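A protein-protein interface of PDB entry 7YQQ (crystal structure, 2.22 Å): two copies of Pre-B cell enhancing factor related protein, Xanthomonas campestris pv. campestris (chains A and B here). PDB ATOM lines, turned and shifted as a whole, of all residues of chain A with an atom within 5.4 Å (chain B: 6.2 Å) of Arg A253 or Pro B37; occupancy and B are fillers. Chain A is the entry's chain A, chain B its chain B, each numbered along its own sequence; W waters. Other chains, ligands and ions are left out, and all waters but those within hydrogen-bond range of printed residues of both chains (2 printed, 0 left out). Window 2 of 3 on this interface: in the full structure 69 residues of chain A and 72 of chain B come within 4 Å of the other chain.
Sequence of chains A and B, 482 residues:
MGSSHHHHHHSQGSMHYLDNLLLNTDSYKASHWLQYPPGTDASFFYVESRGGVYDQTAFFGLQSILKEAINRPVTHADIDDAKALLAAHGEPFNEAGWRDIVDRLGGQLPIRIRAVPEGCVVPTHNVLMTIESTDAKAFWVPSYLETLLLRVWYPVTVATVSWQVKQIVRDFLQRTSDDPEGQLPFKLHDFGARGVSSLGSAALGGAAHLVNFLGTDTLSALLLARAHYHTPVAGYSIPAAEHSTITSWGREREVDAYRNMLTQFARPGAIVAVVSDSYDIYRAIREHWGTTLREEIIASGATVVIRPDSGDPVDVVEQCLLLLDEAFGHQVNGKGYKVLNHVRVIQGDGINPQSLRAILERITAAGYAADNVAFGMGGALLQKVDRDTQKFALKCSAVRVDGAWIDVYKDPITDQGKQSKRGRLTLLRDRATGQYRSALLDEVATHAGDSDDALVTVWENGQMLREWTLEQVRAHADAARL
OG1 of Thr A245 is in hydrogen-bond range of OE1 of Gln B35, 3.1 Å away.
The indole nitrogen (NE1) of Trp A249 is in hydrogen-bond range of the backbone carbonyl oxygen (O) of Gln B35 (2.8 Å).
The backbone carbonyl oxygen (O) of Thr A245 lies within hydrogen-bond range of the side-chain hydroxyl (OG) of Ser A248 (3.1 Å).
NE1 of Trp A249 sits close to O of Thr A245, at 3.5 Å.
The backbone carbonyl oxygen (O) of Trp A249 is in hydrogen-bond range of the guanidinium group (NE) of Arg A253, at 3.5 Å.
The backbone carbonyl oxygen (O) of Pro B37 sits at hydrogen-bond distance from the side-chain hydroxyl (OG1) of Thr B40 (2.8 Å).
N of Ile B406 lies within hydrogen-bond range of O of Val B399.
CG2 of Thr A245 touches CE2 of Tyr B36, 3.9 Å away.
Pro B37 touches Ser A248 (CD to OG, 3.6 Å).
Ser A248 touches Val B399 (CB to CG2, 3.9 Å).
O of Ser A248 touches CD1 of Ile B406, 3.7 Å away.
CZ2 of Trp A249 touches O of Tyr B36, 3.6 Å away.
Trp A249 touches Pro B37 (NE1 to N, 3.5 Å).
Pro B38 touches Trp A249.
Pro B37 touches Arg A253.
Of the printed residues of chain B, Thr A245 touches Gln B35 (3.1 Å) and Tyr B36 (3.9 Å).
Printed residues of chain B within 4 Å of Trp A249: Gln B35, Tyr B36, Pro B37 and Pro B38.
Of chain B, only Pro B37 comes within 4 Å of Arg A253.
Ala A257 touches none of the printed residues of chain B.
Pro B37 touches just these residues of chain A: Ser A248 (3.6 Å), Trp A249 (3.5 Å) and Arg A253 (3.6 Å).
Printed residues of chain A within 4 Å of Pro B38: Trp A249 (3.9 Å).
Printed residues of chain A within 4 Å of Ile B406: Ser A248 (3.7 Å).
The nearest residue of chain B that does not touch Arg A253 is Pro B38 (4.3 Å).
The nearest residue of chain A that does not touch Pro B37 is Thr A245 (4.7 Å).
Of the 11 printed residues of chain B, 6 touch a printed residue of chain A.
Of the 11 printed residues of chain A, 4 touch a printed residue of chain B.
Hydrophobic or aromatic side chains of chain A that line the printed part of chain B: Trp A249.
Among the printed residues, 10 pairs touch across the chains.
Among the printed residues, no Asp or Glu carboxylate lies within 4 Å of a Lys or Arg side-chain nitrogen of the other chain.
No position is printed for both chains.
Water W2 bridges O of Pro B38 and NH2 of Arg A253.
Water W1 lies within hydrogen-bond range of O of Ala A257 (2.9 Å) and O of Gln B35 (3.5 Å).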
ATOM      1  N   THR A 245       4.468 -24.804 -33.701  1.00  0.00           N
ATOM      2  CA  THR A 245       3.967 -24.307 -32.418  1.00  0.00           C
ATOM      3  C   THR A 245       3.061 -23.083 -32.577  1.00  0.00           C
ATOM      4  O   THR A 245       2.006 -23.005 -31.936  1.00  0.00           O
ATOM      5  CB  THR A 245       5.118 -23.979 -31.464  1.00  0.00           C
ATOM      6  OG1 THR A 245       6.227 -23.405 -32.174  1.00  0.00           O
ATOM      7  CG2 THR A 245       5.546 -25.223 -30.720  1.00  0.00           C
ATOM      8  N   SER A 248      -0.552 -23.949 -34.312  1.00  0.00           N
ATOM      9  CA  SER A 248      -1.352 -24.802 -33.430  1.00  0.00           C
ATOM     10  C   SER A 248      -2.050 -24.045 -32.303  1.00  0.00           C
ATOM     11  O   SER A 248      -2.935 -24.613 -31.654  1.00  0.00           O
ATOM     12  CB  SER A 248      -0.480 -25.914 -32.840  1.00  0.00           C
ATOM     13  OG  SER A 248       0.228 -25.487 -31.688  1.00  0.00           O
ATOM     14  N   TRP A 249      -1.693 -22.788 -32.041  1.00  0.00           N
ATOM     15  CA  TRP A 249      -2.507 -22.011 -31.113  1.00  0.00           C
ATOM     16  C   TRP A 249      -3.848 -21.635 -31.722  1.00  0.00           C
ATOM     17  O   TRP A 249      -4.770 -21.282 -30.981  1.00  0.00           O
ATOM     18  CB  TRP A 249      -1.786 -20.734 -30.682  1.00  0.00           C
ATOM     19  CG  TRP A 249      -0.653 -20.946 -29.721  1.00  0.00           C
ATOM     20  CD1 TRP A 249       0.507 -21.596 -29.968  1.00  0.00           C
ATOM     21  CD2 TRP A 249      -0.575 -20.486 -28.366  1.00  0.00           C
ATOM     22  NE1 TRP A 249       1.311 -21.585 -28.850  1.00  0.00           N
ATOM     23  CE2 TRP A 249       0.671 -20.906 -27.852  1.00  0.00           C
ATOM     24  CE3 TRP A 249      -1.434 -19.762 -27.540  1.00  0.00           C
ATOM     25  CZ2 TRP A 249       1.085 -20.623 -26.546  1.00  0.00           C
ATOM     26  CZ3 TRP A 249      -1.019 -19.477 -26.234  1.00  0.00           C
ATOM     27  CH2 TRP A 249       0.228 -19.917 -25.750  1.00  0.00           C
ATOM     28  N   GLY A 250      -3.972 -21.712 -33.041  1.00  0.00           N
ATOM     29  CA  GLY A 250      -5.121 -21.182 -33.755  1.00  0.00           C
ATOM     30  C   GLY A 250      -4.897 -19.753 -34.205  1.00  0.00           C
ATOM     31  O   GLY A 250      -4.119 -18.996 -33.620  1.00  0.00           O
ATOM     32  N   ARG A 251      -5.593 -19.378 -35.284  1.00  0.00           N
ATOM     33  CA  ARG A 251      -5.440 -18.026 -35.825  1.00  0.00           C
ATOM     34  C   ARG A 251      -6.010 -16.971 -34.886  1.00  0.00           C
ATOM     35  O   ARG A 251      -5.536 -15.831 -34.880  1.00  0.00           O
ATOM     36  CB  ARG A 251      -6.102 -17.922 -37.202  1.00  0.00           C
ATOM     37  CG  ARG A 251      -5.316 -18.589 -38.332  1.00  0.00           C
ATOM     38  CD  ARG A 251      -4.281 -17.648 -38.958  1.00  0.00           C
ATOM     39  NE  ARG A 251      -4.782 -16.284 -39.121  1.00  0.00           N
ATOM     40  CZ  ARG A 251      -4.086 -15.281 -39.654  1.00  0.00           C
ATOM     41  NH1 ARG A 251      -2.844 -15.480 -40.083  1.00  0.00           N
ATOM     42  NH2 ARG A 251      -4.636 -14.071 -39.762  1.00  0.00           N
ATOM     43  N   GLU A 252      -7.008 -17.330 -34.082  1.00  0.00           N
ATOM     44  CA  GLU A 252      -7.630 -16.383 -33.166  1.00  0.00           C
ATOM     45  C   GLU A 252      -6.777 -16.080 -31.941  1.00  0.00           C
ATOM     46  O   GLU A 252      -7.056 -15.099 -31.241  1.00  0.00           O
ATOM     47  CB  GLU A 252      -8.990 -16.908 -32.720  1.00  0.00           C
ATOM     48  CG  GLU A 252     -10.175 -16.162 -33.308  1.00  0.00           C
ATOM     49  CD  GLU A 252     -11.473 -16.473 -32.579  1.00  0.00           C
ATOM     50  OE1 GLU A 252     -11.875 -17.659 -32.572  1.00  0.00           O
ATOM     51  OE2 GLU A 252     -12.087 -15.537 -32.017  1.00  0.00           O
ATOM     52  N   ARG A 253      -5.764 -16.902 -31.653  1.00  0.00           N
ATOM     53  CA  ARG A 253      -4.846 -16.669 -30.541  1.00  0.00           C
ATOM     54  C   ARG A 253      -3.403 -16.576 -31.020  1.00  0.00           C
ATOM     55  O   ARG A 253      -2.474 -16.670 -30.205  1.00  0.00           O
ATOM     56  CB  ARG A 253      -4.984 -17.771 -29.489  1.00  0.00           C
ATOM     57  CG  ARG A 253      -6.263 -17.725 -28.678  1.00  0.00           C
ATOM     58  CD  ARG A 253      -6.167 -18.663 -27.498  1.00  0.00           C
ATOM     59  NE  ARG A 253      -5.872 -20.034 -27.924  1.00  0.00           N
ATOM     60  CZ  ARG A 253      -5.318 -20.965 -27.148  1.00  0.00           C
ATOM     61  NH1 ARG A 253      -4.990 -20.679 -25.892  1.00  0.00           N
ATOM     62  NH2 ARG A 253      -5.101 -22.186 -27.624  1.00  0.00           N
ATOM     63  N   GLU A 254      -3.210 -16.396 -32.334  1.00  0.00           N
ATOM     64  CA  GLU A 254      -1.875 -16.387 -32.923  1.00  0.00           C
ATOM     65  C   GLU A 254      -0.967 -15.383 -32.228  1.00  0.00           C
ATOM     66  O   GLU A 254       0.209 -15.667 -31.975  1.00  0.00           O
ATOM     67  CB  GLU A 254      -1.978 -16.076 -34.413  1.00  0.00           C
ATOM     68  CG  GLU A 254      -0.697 -16.298 -35.191  1.00  0.00           C
ATOM     69  CD  GLU A 254      -0.607 -15.425 -36.437  1.00  0.00           C
ATOM     70  OE1 GLU A 254       0.228 -15.739 -37.317  1.00  0.00           O
ATOM     71  OE2 GLU A 254      -1.369 -14.429 -36.535  1.00  0.00           O
ATOM     72  N   VAL A 255      -1.503 -14.211 -31.889  1.00  0.00           N
ATOM     73  CA  VAL A 255      -0.713 -13.212 -31.179  1.00  0.00           C
ATOM     74  C   VAL A 255      -0.299 -13.726 -29.806  1.00  0.00           C
ATOM     75  O   VAL A 255       0.799 -13.414 -29.328  1.00  0.00           O
ATOM     76  CB  VAL A 255      -1.499 -11.880 -31.108  1.00  0.00           C
ATOM     77  CG1 VAL A 255      -1.054 -11.030 -29.928  1.00  0.00           C
ATOM     78  CG2 VAL A 255      -1.322 -11.093 -32.407  1.00  0.00           C
ATOM     79  N   ASP A 256      -1.154 -14.528 -29.155  1.00  0.00           N
ATOM     80  CA  ASP A 256      -0.809 -15.086 -27.846  1.00  0.00           C
ATOM     81  C   ASP A 256       0.359 -16.073 -27.927  1.00  0.00           C
ATOM     82  O   ASP A 256       1.137 -16.183 -26.974  1.00  0.00           O
ATOM     83  CB  ASP A 256      -2.021 -15.772 -27.222  1.00  0.00           C
ATOM     84  CG  ASP A 256      -3.055 -14.784 -26.731  1.00  0.00           C
ATOM     85  OD1 ASP A 256      -2.667 -13.677 -26.301  1.00  0.00           O
ATOM     86  OD2 ASP A 256      -4.256 -15.113 -26.782  1.00  0.00           O
ATOM     87  N   ALA A 257       0.499 -16.801 -29.036  1.00  0.00           N
ATOM     88  CA  ALA A 257       1.703 -17.604 -29.218  1.00  0.00           C
ATOM     89  C   ALA A 257       2.949 -16.726 -29.192  1.00  0.00           C
ATOM     90  O   ALA A 257       3.938 -17.061 -28.530  1.00  0.00           O
ATOM     91  CB  ALA A 257       1.632 -18.396 -30.523  1.00  0.00           C
ATOM     92  N   GLN B  35       6.411 -23.809 -26.076  1.00  0.00           N
ATOM     93  CA  GLN B  35       5.735 -22.995 -27.073  1.00  0.00           C
ATOM     94  C   GLN B  35       4.358 -23.525 -27.467  1.00  0.00           C
ATOM     95  O   GLN B  35       3.671 -22.888 -28.274  1.00  0.00           O
ATOM     96  CB  GLN B  35       6.627 -22.867 -28.316  1.00  0.00           C
ATOM     97  CG  GLN B  35       8.037 -22.426 -27.985  1.00  0.00           C
ATOM     98  CD  GLN B  35       8.923 -22.330 -29.211  1.00  0.00           C
ATOM     99  OE1 GLN B  35       8.442 -22.408 -30.328  1.00  0.00           O
ATOM    100  NE2 GLN B  35      10.226 -22.163 -29.003  1.00  0.00           N
ATOM    101  N   TYR B  36       3.939 -24.661 -26.934  1.00  0.00           N
ATOM    102  CA  TYR B  36       2.605 -25.144 -27.232  1.00  0.00           C
ATOM    103  C   TYR B  36       1.574 -24.405 -26.386  1.00  0.00           C
ATOM    104  O   TYR B  36       1.895 -23.908 -25.303  1.00  0.00           O
ATOM    105  CB  TYR B  36       2.510 -26.639 -26.954  1.00  0.00           C
ATOM    106  CG  TYR B  36       3.195 -27.461 -27.997  1.00  0.00           C
ATOM    107  CD1 TYR B  36       2.535 -27.821 -29.160  1.00  0.00           C
ATOM    108  CD2 TYR B  36       4.508 -27.869 -27.828  1.00  0.00           C
ATOM    109  CE1 TYR B  36       3.162 -28.583 -30.135  1.00  0.00           C
ATOM    110  CE2 TYR B  36       5.140 -28.630 -28.787  1.00  0.00           C
ATOM    111  CZ  TYR B  36       4.459 -28.986 -29.937  1.00  0.00           C
ATOM    112  OH  TYR B  36       5.083 -29.709 -30.894  1.00  0.00           O
ATOM    113  N   PRO B  37       0.330 -24.327 -26.854  1.00  0.00           N
ATOM    114  CA  PRO B  37      -0.732 -23.696 -26.053  1.00  0.00           C
ATOM    115  C   PRO B  37      -0.992 -24.492 -24.788  1.00  0.00           C
ATOM    116  O   PRO B  37      -0.690 -25.693 -24.743  1.00  0.00           O
ATOM    117  CB  PRO B  37      -1.947 -23.726 -26.990  1.00  0.00           C
ATOM    118  CG  PRO B  37      -1.647 -24.794 -27.991  1.00  0.00           C
ATOM    119  CD  PRO B  37      -0.155 -24.775 -28.172  1.00  0.00           C
ATOM    120  N   PRO B  38      -1.528 -23.861 -23.738  1.00  0.00           N
ATOM    121  CA  PRO B  38      -1.881 -24.605 -22.520  1.00  0.00           C
ATOM    122  C   PRO B  38      -2.870 -25.727 -22.805  1.00  0.00           C
ATOM    123  O   PRO B  38      -3.753 -25.614 -23.659  1.00  0.00           O
ATOM    124  CB  PRO B  38      -2.520 -23.538 -21.620  1.00  0.00           C
ATOM    125  CG  PRO B  38      -1.988 -22.257 -22.106  1.00  0.00           C
ATOM    126  CD  PRO B  38      -1.809 -22.419 -23.596  1.00  0.00           C
ATOM    127  N   GLY B  39      -2.742 -26.806 -22.042  1.00  0.00           N
ATOM    128  CA  GLY B  39      -3.613 -27.946 -22.222  1.00  0.00           C
ATOM    129  C   GLY B  39      -3.303 -28.811 -23.424  1.00  0.00           C
ATOM    130  O   GLY B  39      -4.122 -29.658 -23.773  1.00  0.00           O
ATOM    131  N   THR B  40      -2.161 -28.621 -24.085  1.00  0.00           N
ATOM    132  CA  THR B  40      -1.781 -29.525 -25.168  1.00  0.00           C
ATOM    133  C   THR B  40      -1.337 -30.859 -24.579  1.00  0.00           C
ATOM    134  O   THR B  40      -0.482 -30.898 -23.679  1.00  0.00           O
ATOM    135  CB  THR B  40      -0.645 -28.935 -26.016  1.00  0.00           C
ATOM    136  OG1 THR B  40      -1.064 -27.702 -26.609  1.00  0.00           O
ATOM    137  CG2 THR B  40      -0.247 -29.915 -27.110  1.00  0.00           C
ATOM    138  N   PHE B 139       3.863 -35.207 -24.792  1.00  0.00           N
ATOM    139  CA  PHE B 139       3.325 -34.975 -26.134  1.00  0.00           C
ATOM    140  C   PHE B 139       4.319 -34.328 -27.088  1.00  0.00           C
ATOM    141  O   PHE B 139       4.137 -34.426 -28.304  1.00  0.00           O
ATOM    142  CB  PHE B 139       2.102 -34.062 -26.050  1.00  0.00           C
ATOM    143  CG  PHE B 139       2.434 -32.669 -25.606  1.00  0.00           C
ATOM    144  CD1 PHE B 139       2.521 -32.359 -24.244  1.00  0.00           C
ATOM    145  CD2 PHE B 139       2.684 -31.684 -26.527  1.00  0.00           C
ATOM    146  CE1 PHE B 139       2.840 -31.095 -23.820  1.00  0.00           C
ATOM    147  CE2 PHE B 139       3.025 -30.398 -26.108  1.00  0.00           C
ATOM    148  CZ  PHE B 139       3.105 -30.107 -24.749  1.00  0.00           C
ATOM    149  N   VAL B 399      -2.945 -31.490 -33.266  1.00  0.00           N
ATOM    150  CA  VAL B 399      -2.564 -31.513 -31.856  1.00  0.00           C
ATOM    151  C   VAL B 399      -3.841 -31.724 -31.058  1.00  0.00           C
ATOM    152  O   VAL B 399      -4.937 -31.388 -31.521  1.00  0.00           O
ATOM    153  CB  VAL B 399      -1.845 -30.212 -31.381  1.00  0.00           C
ATOM    154  CG1 VAL B 399      -0.486 -30.092 -32.001  1.00  0.00           C
ATOM    155  CG2 VAL B 399      -2.675 -28.984 -31.683  1.00  0.00           C
ATOM    156  N   VAL B 401      -5.745 -30.560 -27.688  1.00  0.00           N
ATOM    157  CA  VAL B 401      -5.753 -29.432 -26.762  1.00  0.00           C
ATOM    158  C   VAL B 401      -7.053 -29.477 -25.977  1.00  0.00           C
ATOM    159  O   VAL B 401      -8.135 -29.550 -26.568  1.00  0.00           O
ATOM    160  CB  VAL B 401      -5.620 -28.077 -27.487  1.00  0.00           C
ATOM    161  CG1 VAL B 401      -5.586 -26.908 -26.478  1.00  0.00           C
ATOM    162  CG2 VAL B 401      -4.377 -28.056 -28.383  1.00  0.00           C
ATOM    163  N   ASP B 402      -6.945 -29.431 -24.650  1.00  0.00           N
ATOM    164  CA  ASP B 402      -8.116 -29.461 -23.770  1.00  0.00           C
ATOM    165  C   ASP B 402      -9.034 -30.630 -24.121  1.00  0.00           C
ATOM    166  O   ASP B 402     -10.261 -30.504 -24.135  1.00  0.00           O
ATOM    167  CB  ASP B 402      -8.868 -28.124 -23.815  1.00  0.00           C
ATOM    168  CG  ASP B 402      -8.068 -26.981 -23.186  1.00  0.00           C
ATOM    169  OD1 ASP B 402      -7.542 -27.182 -22.066  1.00  0.00           O
ATOM    170  OD2 ASP B 402      -7.953 -25.897 -23.814  1.00  0.00           O
ATOM    171  N   ILE B 406      -7.418 -30.902 -32.818  1.00  0.00           N
ATOM    172  CA  ILE B 406      -7.624 -29.807 -33.754  1.00  0.00           C
ATOM    173  C   ILE B 406      -6.641 -29.951 -34.913  1.00  0.00           C
ATOM    174  O   ILE B 406      -5.490 -30.363 -34.727  1.00  0.00           O
ATOM    175  CB  ILE B 406      -7.522 -28.415 -33.076  1.00  0.00           C
ATOM    176  CG1 ILE B 406      -6.084 -27.994 -32.798  1.00  0.00           C
ATOM    177  CG2 ILE B 406      -8.309 -28.366 -31.765  1.00  0.00           C
ATOM    178  CD1 ILE B 406      -5.973 -26.762 -31.874  1.00  0.00           C
HETATM  179  O   HOH W   1       4.940 -19.687 -27.821  1.00  0.00           O
HETATM  180  O   HOH W   2      -5.445 -23.670 -24.837  1.00  0.00           O
